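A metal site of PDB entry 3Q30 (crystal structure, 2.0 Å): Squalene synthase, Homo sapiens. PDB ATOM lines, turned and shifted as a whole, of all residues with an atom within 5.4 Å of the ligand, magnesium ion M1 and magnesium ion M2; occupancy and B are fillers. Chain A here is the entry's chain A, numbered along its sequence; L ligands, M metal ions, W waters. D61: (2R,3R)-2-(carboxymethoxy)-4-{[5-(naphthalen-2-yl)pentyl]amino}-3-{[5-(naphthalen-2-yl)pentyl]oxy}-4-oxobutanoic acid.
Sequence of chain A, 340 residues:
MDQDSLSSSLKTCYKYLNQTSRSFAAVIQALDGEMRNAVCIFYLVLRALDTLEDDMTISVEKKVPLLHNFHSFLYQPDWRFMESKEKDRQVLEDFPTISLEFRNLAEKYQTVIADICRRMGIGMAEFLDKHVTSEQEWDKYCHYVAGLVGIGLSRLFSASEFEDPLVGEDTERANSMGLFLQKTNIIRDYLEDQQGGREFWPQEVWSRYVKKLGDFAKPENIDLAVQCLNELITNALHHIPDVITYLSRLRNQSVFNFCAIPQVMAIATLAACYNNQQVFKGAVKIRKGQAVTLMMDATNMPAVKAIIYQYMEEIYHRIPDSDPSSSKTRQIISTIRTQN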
ATOM      1  N   ILE A  28      22.473  26.188 -27.627  1.00  0.00           N
ATOM      2  CA  ILE A  28      22.532  24.781 -27.242  1.00  0.00           C
ATOM      3  C   ILE A  28      22.999  23.902 -28.421  1.00  0.00           C
ATOM      4  O   ILE A  28      23.898  23.085 -28.271  1.00  0.00           O
ATOM      5  CB  ILE A  28      21.190  24.268 -26.612  1.00  0.00           C
ATOM      6  CG1 ILE A  28      20.988  24.946 -25.246  1.00  0.00           C
ATOM      7  CG2 ILE A  28      21.215  22.729 -26.467  1.00  0.00           C
ATOM      8  CD1 ILE A  28      19.640  24.704 -24.562  1.00  0.00           C
ATOM      9  N   VAL A  39      22.745  18.697 -22.818  1.00  0.00           N
ATOM     10  CA  VAL A  39      22.174  19.974 -22.394  1.00  0.00           C
ATOM     11  C   VAL A  39      20.766  20.096 -22.992  1.00  0.00           C
ATOM     12  O   VAL A  39      19.841  20.609 -22.333  1.00  0.00           O
ATOM     13  CB  VAL A  39      23.138  21.185 -22.766  1.00  0.00           C
ATOM     14  CG1 VAL A  39      22.423  22.533 -22.696  1.00  0.00           C
ATOM     15  CG2 VAL A  39      24.379  21.181 -21.926  1.00  0.00           C
ATOM     16  N   PHE A  42      18.722  18.003 -20.627  1.00  0.00           N
ATOM     17  CA  PHE A  42      18.665  18.676 -19.291  1.00  0.00           C
ATOM     18  C   PHE A  42      17.652  19.836 -19.283  1.00  0.00           C
ATOM     19  O   PHE A  42      16.935  20.098 -18.281  1.00  0.00           O
ATOM     20  CB  PHE A  42      20.064  19.223 -18.970  1.00  0.00           C
ATOM     21  CG  PHE A  42      20.228  19.745 -17.562  1.00  0.00           C
ATOM     22  CD1 PHE A  42      21.088  20.798 -17.326  1.00  0.00           C
ATOM     23  CD2 PHE A  42      19.617  19.121 -16.482  1.00  0.00           C
ATOM     24  CE1 PHE A  42      21.272  21.283 -16.026  1.00  0.00           C
ATOM     25  CE2 PHE A  42      19.809  19.604 -15.188  1.00  0.00           C
ATOM     26  CZ  PHE A  42      20.643  20.673 -14.973  1.00  0.00           C
ATOM     27  N   TYR A  43      17.668  20.566 -20.392  1.00  0.00           N
ATOM     28  CA  TYR A  43      16.743  21.666 -20.578  1.00  0.00           C
ATOM     29  C   TYR A  43      15.304  21.184 -20.521  1.00  0.00           C
ATOM     30  O   TYR A  43      14.504  21.705 -19.746  1.00  0.00           O
ATOM     31  CB  TYR A  43      16.980  22.394 -21.900  1.00  0.00           C
ATOM     32  CG  TYR A  43      16.010  23.534 -22.041  1.00  0.00           C
ATOM     33  CD1 TYR A  43      14.777  23.348 -22.686  1.00  0.00           C
ATOM     34  CD2 TYR A  43      16.276  24.774 -21.445  1.00  0.00           C
ATOM     35  CE1 TYR A  43      13.859  24.373 -22.762  1.00  0.00           C
ATOM     36  CE2 TYR A  43      15.344  25.825 -21.513  1.00  0.00           C
ATOM     37  CZ  TYR A  43      14.149  25.599 -22.180  1.00  0.00           C
ATOM     38  OH  TYR A  43      13.227  26.605 -22.286  1.00  0.00           O
ATOM     39  N   LEU A  46      14.129  19.867 -17.140  1.00  0.00           N
ATOM     40  CA  LEU A  46      13.862  20.864 -16.090  1.00  0.00           C
ATOM     41  C   LEU A  46      12.723  21.773 -16.477  1.00  0.00           C
ATOM     42  O   LEU A  46      12.006  22.263 -15.592  1.00  0.00           O
ATOM     43  CB  LEU A  46      15.091  21.696 -15.742  1.00  0.00           C
ATOM     44  CG  LEU A  46      16.240  20.898 -15.139  1.00  0.00           C
ATOM     45  CD1 LEU A  46      17.381  21.838 -14.929  1.00  0.00           C
ATOM     46  CD2 LEU A  46      15.857  20.176 -13.804  1.00  0.00           C
ATOM     47  N   ARG A  47      12.524  21.986 -17.768  1.00  0.00           N
ATOM     48  CA  ARG A  47      11.319  22.705 -18.223  1.00  0.00           C
ATOM     49  C   ARG A  47      10.040  21.912 -17.958  1.00  0.00           C
ATOM     50  O   ARG A  47       9.017  22.517 -17.636  1.00  0.00           O
ATOM     51  CB  ARG A  47      11.413  23.128 -19.687  1.00  0.00           C
ATOM     52  CG  ARG A  47      10.439  24.250 -20.130  1.00  0.00           C
ATOM     53  CD  ARG A  47      10.309  25.455 -19.171  1.00  0.00           C
ATOM     54  NE  ARG A  47      11.495  26.293 -19.225  1.00  0.00           N
ATOM     55  CZ  ARG A  47      11.913  27.126 -18.259  1.00  0.00           C
ATOM     56  NH1 ARG A  47      11.246  27.261 -17.112  1.00  0.00           N
ATOM     57  NH2 ARG A  47      13.018  27.834 -18.453  1.00  0.00           N
ATOM     58  N   ASP A  50       9.510  22.276 -14.263  1.00  0.00           N
ATOM     59  CA  ASP A  50       8.996  23.633 -13.970  1.00  0.00           C
ATOM     60  C   ASP A  50       7.543  23.836 -14.456  1.00  0.00           C
ATOM     61  O   ASP A  50       6.793  24.635 -13.895  1.00  0.00           O
ATOM     62  CB  ASP A  50       9.864  24.730 -14.565  1.00  0.00           C
ATOM     63  CG  ASP A  50       9.409  26.105 -14.112  1.00  0.00           C
ATOM     64  OD1 ASP A  50       9.327  26.356 -12.885  1.00  0.00           O
ATOM     65  OD2 ASP A  50       9.105  26.925 -14.996  1.00  0.00           O
ATOM     66  N   GLU A  53       5.527  22.637 -11.722  1.00  0.00           N
ATOM     67  CA  GLU A  53       5.624  23.611 -10.627  1.00  0.00           C
ATOM     68  C   GLU A  53       4.789  24.874 -10.899  1.00  0.00           C
ATOM     69  O   GLU A  53       4.130  25.368  -9.993  1.00  0.00           O
ATOM     70  CB  GLU A  53       7.101  24.005 -10.373  1.00  0.00           C
ATOM     71  CG  GLU A  53       7.298  24.660  -8.998  1.00  0.00           C
ATOM     72  CD  GLU A  53       7.952  26.014  -9.084  1.00  0.00           C
ATOM     73  OE1 GLU A  53       7.784  26.641 -10.145  1.00  0.00           O
ATOM     74  OE2 GLU A  53       8.623  26.461  -8.111  1.00  0.00           O
ATOM     75  N   ASP A  54       4.812  25.379 -12.122  1.00  0.00           N
ATOM     76  CA  ASP A  54       4.100  26.603 -12.489  1.00  0.00           C
ATOM     77  C   ASP A  54       2.589  26.372 -12.562  1.00  0.00           C
ATOM     78  O   ASP A  54       1.799  27.306 -12.489  1.00  0.00           O
ATOM     79  CB  ASP A  54       4.600  27.106 -13.839  1.00  0.00           C
ATOM     80  CG  ASP A  54       5.977  27.746 -13.749  1.00  0.00           C
ATOM     81  OD1 ASP A  54       6.515  27.885 -12.634  1.00  0.00           O
ATOM     82  OD2 ASP A  54       6.528  28.077 -14.812  1.00  0.00           O
ATOM     83  N   MET A 120      16.294  20.175  -7.023  1.00  0.00           N
ATOM     84  CA  MET A 120      15.384  21.245  -7.421  1.00  0.00           C
ATOM     85  C   MET A 120      13.952  20.897  -7.030  1.00  0.00           C
ATOM     86  O   MET A 120      13.169  21.781  -6.630  1.00  0.00           O
ATOM     87  CB  MET A 120      15.464  21.477  -8.955  1.00  0.00           C
ATOM     88  CG  MET A 120      14.446  22.529  -9.494  1.00  0.00           C
ATOM     89  SD  MET A 120      14.658  23.000 -11.244  1.00  0.00           S
ATOM     90  CE  MET A 120      16.481  23.254 -11.265  1.00  0.00           C
ATOM     91  N   MET A 124      11.678  23.267  -4.874  1.00  0.00           N
ATOM     92  CA  MET A 124      10.443  23.770  -5.413  1.00  0.00           C
ATOM     93  C   MET A 124       9.273  23.394  -4.475  1.00  0.00           C
ATOM     94  O   MET A 124       8.420  24.225  -4.191  1.00  0.00           O
ATOM     95  CB  MET A 124      10.200  23.211  -6.808  1.00  0.00           C
ATOM     96  CG  MET A 124      10.957  23.949  -7.921  1.00  0.00           C
ATOM     97  SD  MET A 124      10.702  22.984  -9.385  1.00  0.00           S
ATOM     98  CE  MET A 124      11.273  24.135 -10.687  1.00  0.00           C
ATOM     99  N   TYR A 141      15.524  30.247  -2.641  1.00  0.00           N
ATOM    100  CA  TYR A 141      14.621  30.048  -3.760  1.00  0.00           C
ATOM    101  C   TYR A 141      15.367  30.108  -5.112  1.00  0.00           C
ATOM    102  O   TYR A 141      15.255  29.173  -5.902  1.00  0.00           O
ATOM    103  CB  TYR A 141      13.435  31.052  -3.738  1.00  0.00           C
ATOM    104  CG  TYR A 141      12.588  30.968  -4.985  1.00  0.00           C
ATOM    105  CD1 TYR A 141      11.594  29.972  -5.113  1.00  0.00           C
ATOM    106  CD2 TYR A 141      12.790  31.840  -6.057  1.00  0.00           C
ATOM    107  CE1 TYR A 141      10.835  29.871  -6.249  1.00  0.00           C
ATOM    108  CE2 TYR A 141      12.046  31.736  -7.206  1.00  0.00           C
ATOM    109  CZ  TYR A 141      11.060  30.742  -7.293  1.00  0.00           C
ATOM    110  OH  TYR A 141      10.292  30.644  -8.440  1.00  0.00           O
ATOM    111  N   VAL A 145      15.822  27.037  -7.997  1.00  0.00           N
ATOM    112  CA  VAL A 145      15.200  27.038  -9.317  1.00  0.00           C
ATOM    113  C   VAL A 145      16.143  27.455 -10.445  1.00  0.00           C
ATOM    114  O   VAL A 145      15.841  27.235 -11.616  1.00  0.00           O
ATOM    115  CB  VAL A 145      13.849  27.897  -9.385  1.00  0.00           C
ATOM    116  CG1 VAL A 145      12.854  27.423  -8.288  1.00  0.00           C
ATOM    117  CG2 VAL A 145      14.117  29.400  -9.280  1.00  0.00           C
ATOM    118  N   ALA A 146      17.283  28.055 -10.085  1.00  0.00           N
ATOM    119  CA  ALA A 146      18.183  28.633 -11.089  1.00  0.00           C
ATOM    120  C   ALA A 146      19.673  28.342 -10.803  1.00  0.00           C
ATOM    121  O   ALA A 146      20.465  28.023 -11.714  1.00  0.00           O
ATOM    122  CB  ALA A 146      17.956  30.140 -11.181  1.00  0.00           C
ATOM    123  N   VAL A 149      20.560  24.894 -11.782  1.00  0.00           N
ATOM    124  CA  VAL A 149      20.739  24.754 -13.260  1.00  0.00           C
ATOM    125  C   VAL A 149      22.193  25.073 -13.648  1.00  0.00           C
ATOM    126  O   VAL A 149      22.845  24.297 -14.364  1.00  0.00           O
ATOM    127  CB  VAL A 149      19.799  25.657 -14.074  1.00  0.00           C
ATOM    128  CG1 VAL A 149      20.004  25.395 -15.626  1.00  0.00           C
ATOM    129  CG2 VAL A 149      18.368  25.356 -13.727  1.00  0.00           C
ATOM    130  N   GLY A 150      22.719  26.187 -13.131  1.00  0.00           N
ATOM    131  CA  GLY A 150      24.151  26.506 -13.274  1.00  0.00           C
ATOM    132  C   GLY A 150      25.059  25.388 -12.815  1.00  0.00           C
ATOM    133  O   GLY A 150      26.067  25.051 -13.477  1.00  0.00           O
ATOM    134  N   LEU A 153      24.685  22.313 -15.279  1.00  0.00           N
ATOM    135  CA  LEU A 153      25.379  22.626 -16.530  1.00  0.00           C
ATOM    136  C   LEU A 153      26.872  22.555 -16.355  1.00  0.00           C
ATOM    137  O   LEU A 153      27.587  21.899 -17.176  1.00  0.00           O
ATOM    138  CB  LEU A 153      24.985  24.022 -17.045  1.00  0.00           C
ATOM    139  CG  LEU A 153      23.541  24.097 -17.528  1.00  0.00           C
ATOM    140  CD1 LEU A 153      23.154  25.572 -17.644  1.00  0.00           C
ATOM    141  CD2 LEU A 153      23.442  23.398 -18.899  1.00  0.00           C
ATOM    142  N   PHE A 157      29.688  20.184 -18.351  1.00  0.00           N
ATOM    143  CA  PHE A 157      30.889  20.704 -19.008  1.00  0.00           C
ATOM    144  C   PHE A 157      32.086  19.934 -18.516  1.00  0.00           C
ATOM    145  O   PHE A 157      32.888  19.490 -19.344  1.00  0.00           O
ATOM    146  CB  PHE A 157      31.102  22.234 -18.818  1.00  0.00           C
ATOM    147  CG  PHE A 157      29.887  23.121 -19.209  1.00  0.00           C
ATOM    148  CD1 PHE A 157      29.685  24.320 -18.542  1.00  0.00           C
ATOM    149  CD2 PHE A 157      29.001  22.778 -20.217  1.00  0.00           C
ATOM    150  CE1 PHE A 157      28.636  25.161 -18.862  1.00  0.00           C
ATOM    151  CE2 PHE A 157      27.909  23.618 -20.542  1.00  0.00           C
ATOM    152  CZ  PHE A 157      27.751  24.815 -19.836  1.00  0.00           C
ATOM    153  N   ALA A 174      29.011  28.898 -10.135  1.00  0.00           N
ATOM    154  CA  ALA A 174      27.925  28.380 -10.932  1.00  0.00           C
ATOM    155  C   ALA A 174      26.572  28.789 -10.342  1.00  0.00           C
ATOM    156  O   ALA A 174      25.671  29.143 -11.068  1.00  0.00           O
ATOM    157  CB  ALA A 174      28.017  26.865 -11.031  1.00  0.00           C
ATOM    158  N   MET A 177      25.886  32.397 -11.319  1.00  0.00           N
ATOM    159  CA  MET A 177      25.423  32.516 -12.692  1.00  0.00           C
ATOM    160  C   MET A 177      23.895  32.410 -12.807  1.00  0.00           C
ATOM    161  O   MET A 177      23.264  33.152 -13.583  1.00  0.00           O
ATOM    162  CB  MET A 177      26.015  31.422 -13.607  1.00  0.00           C
ATOM    163  CG  MET A 177      27.542  31.464 -13.792  1.00  0.00           C
ATOM    164  SD  MET A 177      28.064  32.748 -14.954  1.00  0.00           S
ATOM    165  CE  MET A 177      27.503  32.042 -16.513  1.00  0.00           C
ATOM    166  N   GLY A 178      23.339  31.421 -12.109  1.00  0.00           N
ATOM    167  CA  GLY A 178      21.866  31.180 -12.213  1.00  0.00           C
ATOM    168  C   GLY A 178      21.099  32.229 -11.414  1.00  0.00           C
ATOM    169  O   GLY A 178      20.060  32.688 -11.814  1.00  0.00           O
ATOM    170  N   LEU A 181      20.691  35.547 -13.451  1.00  0.00           N
ATOM    171  CA  LEU A 181      19.664  35.424 -14.471  1.00  0.00           C
ATOM    172  C   LEU A 181      18.291  35.432 -13.879  1.00  0.00           C
ATOM    173  O   LEU A 181      17.392  36.077 -14.406  1.00  0.00           O
ATOM    174  CB  LEU A 181      19.871  34.160 -15.306  1.00  0.00           C
ATOM    175  CG  LEU A 181      21.172  34.061 -16.133  1.00  0.00           C
ATOM    176  CD1 LEU A 181      21.191  32.703 -16.924  1.00  0.00           C
ATOM    177  CD2 LEU A 181      21.228  35.281 -17.087  1.00  0.00           C
ATOM    178  N   GLN A 182      18.109  34.658 -12.813  1.00  0.00           N
ATOM    179  CA  GLN A 182      16.788  34.503 -12.234  1.00  0.00           C
ATOM    180  C   GLN A 182      16.318  35.763 -11.510  1.00  0.00           C
ATOM    181  O   GLN A 182      15.162  36.113 -11.587  1.00  0.00           O
ATOM    182  CB  GLN A 182      16.759  33.296 -11.252  1.00  0.00           C
ATOM    183  CG  GLN A 182      15.407  33.106 -10.541  1.00  0.00           C
ATOM    184  CD  GLN A 182      14.352  32.481 -11.428  1.00  0.00           C
ATOM    185  OE1 GLN A 182      14.629  32.068 -12.530  1.00  0.00           O
ATOM    186  NE2 GLN A 182      13.129  32.396 -10.913  1.00  0.00           N
ATOM    187  N   ASN A 185      15.221  38.365 -14.109  1.00  0.00           N
ATOM    188  CA  ASN A 185      13.923  37.954 -14.604  1.00  0.00           C
ATOM    189  C   ASN A 185      12.846  38.352 -13.599  1.00  0.00           C
ATOM    190  O   ASN A 185      11.875  38.988 -13.955  1.00  0.00           O
ATOM    191  CB  ASN A 185      13.987  36.418 -14.842  1.00  0.00           C
ATOM    192  CG  ASN A 185      12.832  35.890 -15.608  1.00  0.00           C
ATOM    193  OD1 ASN A 185      12.664  36.169 -16.785  1.00  0.00           O
ATOM    194  ND2 ASN A 185      12.058  35.013 -14.967  1.00  0.00           N
ATOM    195  N   TYR A 246      33.502  33.156 -13.274  1.00  0.00           N
ATOM    196  CA  TYR A 246      33.013  31.938 -13.858  1.00  0.00           C
ATOM    197  C   TYR A 246      33.380  31.891 -15.362  1.00  0.00           C
ATOM    198  O   TYR A 246      33.938  30.896 -15.887  1.00  0.00           O
ATOM    199  CB  TYR A 246      31.462  31.817 -13.696  1.00  0.00           C
ATOM    200  CG  TYR A 246      30.938  30.504 -14.262  1.00  0.00           C
ATOM    201  CD1 TYR A 246      30.603  30.399 -15.603  1.00  0.00           C
ATOM    202  CD2 TYR A 246      30.795  29.355 -13.432  1.00  0.00           C
ATOM    203  CE1 TYR A 246      30.126  29.197 -16.146  1.00  0.00           C
ATOM    204  CE2 TYR A 246      30.309  28.133 -13.964  1.00  0.00           C
ATOM    205  CZ  TYR A 246      29.986  28.070 -15.321  1.00  0.00           C
ATOM    206  OH  TYR A 246      29.550  26.878 -15.865  1.00  0.00           O
ATOM    207  N   PHE A 258      27.639  29.820 -24.926  1.00  0.00           N
ATOM    208  CA  PHE A 258      26.479  29.290 -24.185  1.00  0.00           C
ATOM    209  C   PHE A 258      26.278  29.993 -22.857  1.00  0.00           C
ATOM    210  O   PHE A 258      25.163  30.349 -22.473  1.00  0.00           O
ATOM    211  CB  PHE A 258      26.600  27.757 -23.973  1.00  0.00           C
ATOM    212  CG  PHE A 258      25.450  27.162 -23.185  1.00  0.00           C
ATOM    213  CD1 PHE A 258      25.607  26.825 -21.843  1.00  0.00           C
ATOM    214  CD2 PHE A 258      24.196  26.949 -23.767  1.00  0.00           C
ATOM    215  CE1 PHE A 258      24.549  26.236 -21.104  1.00  0.00           C
ATOM    216  CE2 PHE A 258      23.118  26.409 -23.018  1.00  0.00           C
ATOM    217  CZ  PHE A 258      23.303  26.049 -21.685  1.00  0.00           C
ATOM    218  N   CYS A 259      27.366  30.242 -22.166  1.00  0.00           N
ATOM    219  CA  CYS A 259      27.297  30.787 -20.838  1.00  0.00           C
ATOM    220  C   CYS A 259      27.236  32.307 -20.862  1.00  0.00           C
ATOM    221  O   CYS A 259      26.452  32.876 -20.113  1.00  0.00           O
ATOM    222  CB  CYS A 259      28.481  30.291 -20.013  1.00  0.00           C
ATOM    223  SG  CYS A 259      28.408  28.496 -19.638  1.00  0.00           S
ATOM    224  N   PRO A 262      23.534  34.480 -22.083  1.00  0.00           N
ATOM    225  CA  PRO A 262      22.414  34.850 -21.263  1.00  0.00           C
ATOM    226  C   PRO A 262      22.871  35.915 -20.289  1.00  0.00           C
ATOM    227  O   PRO A 262      22.078  36.801 -19.998  1.00  0.00           O
ATOM    228  CB  PRO A 262      22.023  33.544 -20.525  1.00  0.00           C
ATOM    229  CG  PRO A 262      22.652  32.432 -21.328  1.00  0.00           C
ATOM    230  CD  PRO A 262      23.919  33.053 -21.889  1.00  0.00           C
ATOM    231  N   GLN A 263      24.139  35.874 -19.853  1.00  0.00           N
ATOM    232  CA  GLN A 263      24.618  36.874 -18.895  1.00  0.00           C
ATOM    233  C   GLN A 263      24.596  38.282 -19.491  1.00  0.00           C
ATOM    234  O   GLN A 263      24.108  39.212 -18.846  1.00  0.00           O
ATOM    235  CB  GLN A 263      26.020  36.528 -18.348  1.00  0.00           C
ATOM    236  CG  GLN A 263      26.030  35.120 -17.671  1.00  0.00           C
ATOM    237  CD  GLN A 263      25.211  35.115 -16.393  1.00  0.00           C
ATOM    238  OE1 GLN A 263      25.194  36.128 -15.637  1.00  0.00           O
ATOM    239  NE2 GLN A 263      24.519  34.000 -16.137  1.00  0.00           N
HETATM  240  C1  D61 L   1      25.218  29.037 -17.822  1.00  0.00           C
HETATM  241  C2  D61 L   1      24.395  28.956 -18.977  1.00  0.00           C
HETATM  242  C3  D61 L   1      23.001  28.924 -18.891  1.00  0.00           C
HETATM  243  C4  D61 L   1      22.369  28.990 -17.616  1.00  0.00           C
HETATM  244  C5  D61 L   1      23.200  29.068 -16.451  1.00  0.00           C
HETATM  245  C6  D61 L   1      24.622  29.100 -16.567  1.00  0.00           C
HETATM  246  C7  D61 L   1      22.605  29.100 -15.169  1.00  0.00           C
HETATM  247  C8  D61 L   1      21.217  29.078 -15.030  1.00  0.00           C
HETATM  248  C9  D61 L   1      20.390  28.990 -16.156  1.00  0.00           C
HETATM  249  C10 D61 L   1      20.958  28.945 -17.467  1.00  0.00           C
HETATM  250  C11 D61 L   1      18.885  28.983 -15.924  1.00  0.00           C
HETATM  251  C12 D61 L   1      18.425  30.444 -15.661  1.00  0.00           C
HETATM  252  C13 D61 L   1      16.883  30.535 -15.663  1.00  0.00           C
HETATM  253  C14 D61 L   1      16.363  31.783 -16.426  1.00  0.00           C
HETATM  254  C15 D61 L   1      14.830  31.751 -16.635  1.00  0.00           C
HETATM  255  N16 D61 L   1      14.161  31.268 -15.397  1.00  0.00           N
HETATM  256  C17 D61 L   1      13.418  30.152 -15.395  1.00  0.00           C
HETATM  257  O18 D61 L   1      13.314  29.403 -16.375  1.00  0.00           O
HETATM  258  C19 D61 L   1      12.614  29.805 -14.153  1.00  0.00           C
HETATM  259  O20 D61 L   1      12.493  28.358 -14.052  1.00  0.00           O
HETATM  260  C21 D61 L   1      13.200  27.630 -13.029  1.00  0.00           C
HETATM  261  C22 D61 L   1      13.285  26.126 -13.284  1.00  0.00           C
HETATM  262  C23 D61 L   1      13.322  25.667 -14.772  1.00  0.00           C
HETATM  263  C24 D61 L   1      14.732  25.805 -15.396  1.00  0.00           C
HETATM  264  C25 D61 L   1      14.739  25.412 -16.861  1.00  0.00           C
HETATM  265  C26 D61 L   1      16.022  25.665 -17.674  1.00  0.00           C
HETATM  266  C27 D61 L   1      16.311  26.938 -18.189  1.00  0.00           C
HETATM  267  C28 D61 L   1      17.468  27.145 -18.947  1.00  0.00           C
HETATM  268  C29 D61 L   1      18.311  26.058 -19.214  1.00  0.00           C
HETATM  269  C30 D61 L   1      18.014  24.757 -18.683  1.00  0.00           C
HETATM  270  C31 D61 L   1      16.875  24.567 -17.924  1.00  0.00           C
HETATM  271  C32 D61 L   1      18.856  23.677 -18.937  1.00  0.00           C
HETATM  272  C33 D61 L   1      19.994  23.868 -19.713  1.00  0.00           C
HETATM  273  C34 D61 L   1      20.280  25.127 -20.229  1.00  0.00           C
HETATM  274  C35 D61 L   1      19.458  26.217 -19.986  1.00  0.00           C
HETATM  275  C36 D61 L   1      11.180  30.368 -14.295  1.00  0.00           C
HETATM  276  O37 D61 L   1      10.583  29.763 -15.498  1.00  0.00           O
HETATM  277  C38 D61 L   1      10.214  30.576 -16.681  1.00  0.00           C
HETATM  278  C39 D61 L   1       9.117  29.948 -17.554  1.00  0.00           C
HETATM  279  O40 D61 L   1       9.039  30.334 -18.751  1.00  0.00           O
HETATM  280  O41 D61 L   1       8.372  29.055 -17.031  1.00  0.00           O
HETATM  281  C42 D61 L   1      10.419  30.034 -12.991  1.00  0.00           C
HETATM  282  O43 D61 L   1       9.394  29.301 -13.029  1.00  0.00           O
HETATM  283  O44 D61 L   1      10.891  30.505 -11.914  1.00  0.00           O
HETATM  284 MG    MG M   1       8.611  27.800 -11.620  1.00  0.00          MG
HETATM  285 MG    MG M   2       8.464  28.877 -14.893  1.00  0.00          MG
HETATM  286  O   HOH W   1       7.582  30.587 -14.847  1.00  0.00           O
HETATM  287  O   HOH W   2       7.557  29.620 -10.794  1.00  0.00           O
HETATM  288  O   HOH W   3      10.241  28.076 -10.605  1.00  0.00           O
HETATM  289  O   HOH W   4      10.545  32.711 -10.132  1.00  0.00           O
HETATM  290  O   HOH W   5       5.272  27.463 -17.200  1.00  0.00           O
HETATM  291  O   HOH W   6      24.549  32.113 -18.363  1.00  0.00           O
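The guanidinium group (NH2) of Arg 47 is in hydrogen-bond range of an oxygen (O18) of the ligand (2.6 Å).
The side-chain amide oxygen (OE1) of Gln 182 is in hydrogen-bond range of a nitrogen (N16) of the ligand, at 3.0 Å.
Merely in contact with magnesium ion M2: Arg 47 (3.9 Å).
Of the 29 residues printed, 3 come within 4 Å of magnesium ion M2.
The nearest printed residue that does not touch magnesium ion M2 is Glu 53 (5.3 Å).
Water W3 lies within hydrogen-bond range of an oxygen (O44) of the ligand (2.8 Å), the side-chain hydroxyl (OH) of Tyr 141 (3.4 Å) and the side-chain carboxylate (OE2) of Glu 53 (3.4 Å).
Water W4 lies within hydrogen-bond range of the side-chain hydroxyl (OH) of Tyr 141, the side-chain amide nitrogen (NE2) of Gln 182 and an oxygen (O44) of the ligand.
Water W6 lies within hydrogen-bond range of the backbone carbonyl oxygen of Cys 259 (2.7 Å) and the side-chain amide nitrogen of Gln 263 (2.9 Å).
Water W3 is bound to magnesium ion M1, 1.9 Å away.
OD1 of Asp 50 is bound to magnesium ion M1.
The side-chain carboxylate (OE1) of Glu 53 is bound to magnesium ion M1, 2.1 Å away.
Magnesium ion M1 is bound by O43 of the ligand.
Water W2 is bound to magnesium ion M1 (2.3 Å).
OD1 of Asp 54 is bound to magnesium ion M1, 2.3 Å away.
Magnesium ion M2 is bound by water W1 (1.9 Å), the side-chain carboxylate of Asp 50 (2.1 Å), the side-chain carboxylate of Asp 54 (2.1 Å), an oxygen (O43) of the ligand (2.1 Å), an oxygen (O41) of the ligand (2.1 Å) and an oxygen (O37) of the ligand (2.4 Å).
Magnesium ion M2 has six donor atoms within binding distance.
Merely in contact with the ligand: Phe 42, Tyr 43, Leu 46, Met 120, Met 124, Tyr 141, Val 145, Ala 146, Val 149, Gly 150, Leu 153, Met 177, Gly 178, Leu 181, Phe 258 and Cys 259.
Of the 29 residues printed, 20 come within 4 Å of the ligand.
The nearest printed residue that does not touch the ligand is Val 39 (4.1 Å).
The guanidinium group (NH1) of Arg 47 sits close to the side-chain carboxylate (OD2) of Asp 50 (3.0 Å).
O of Met 177 lies within hydrogen-bond range of NE2 of Gln 263 (3.0 Å).
Three residues have an atom within 4 Å of magnesium ion M1: Asp 50, Glu 53 and Asp 54.
Along chain A the residues within 4 Å of magnesium ion M1 span positions 50 to 54.
The nearest printed residue that does not touch magnesium ion M1 is Tyr 141 (4.6 Å).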
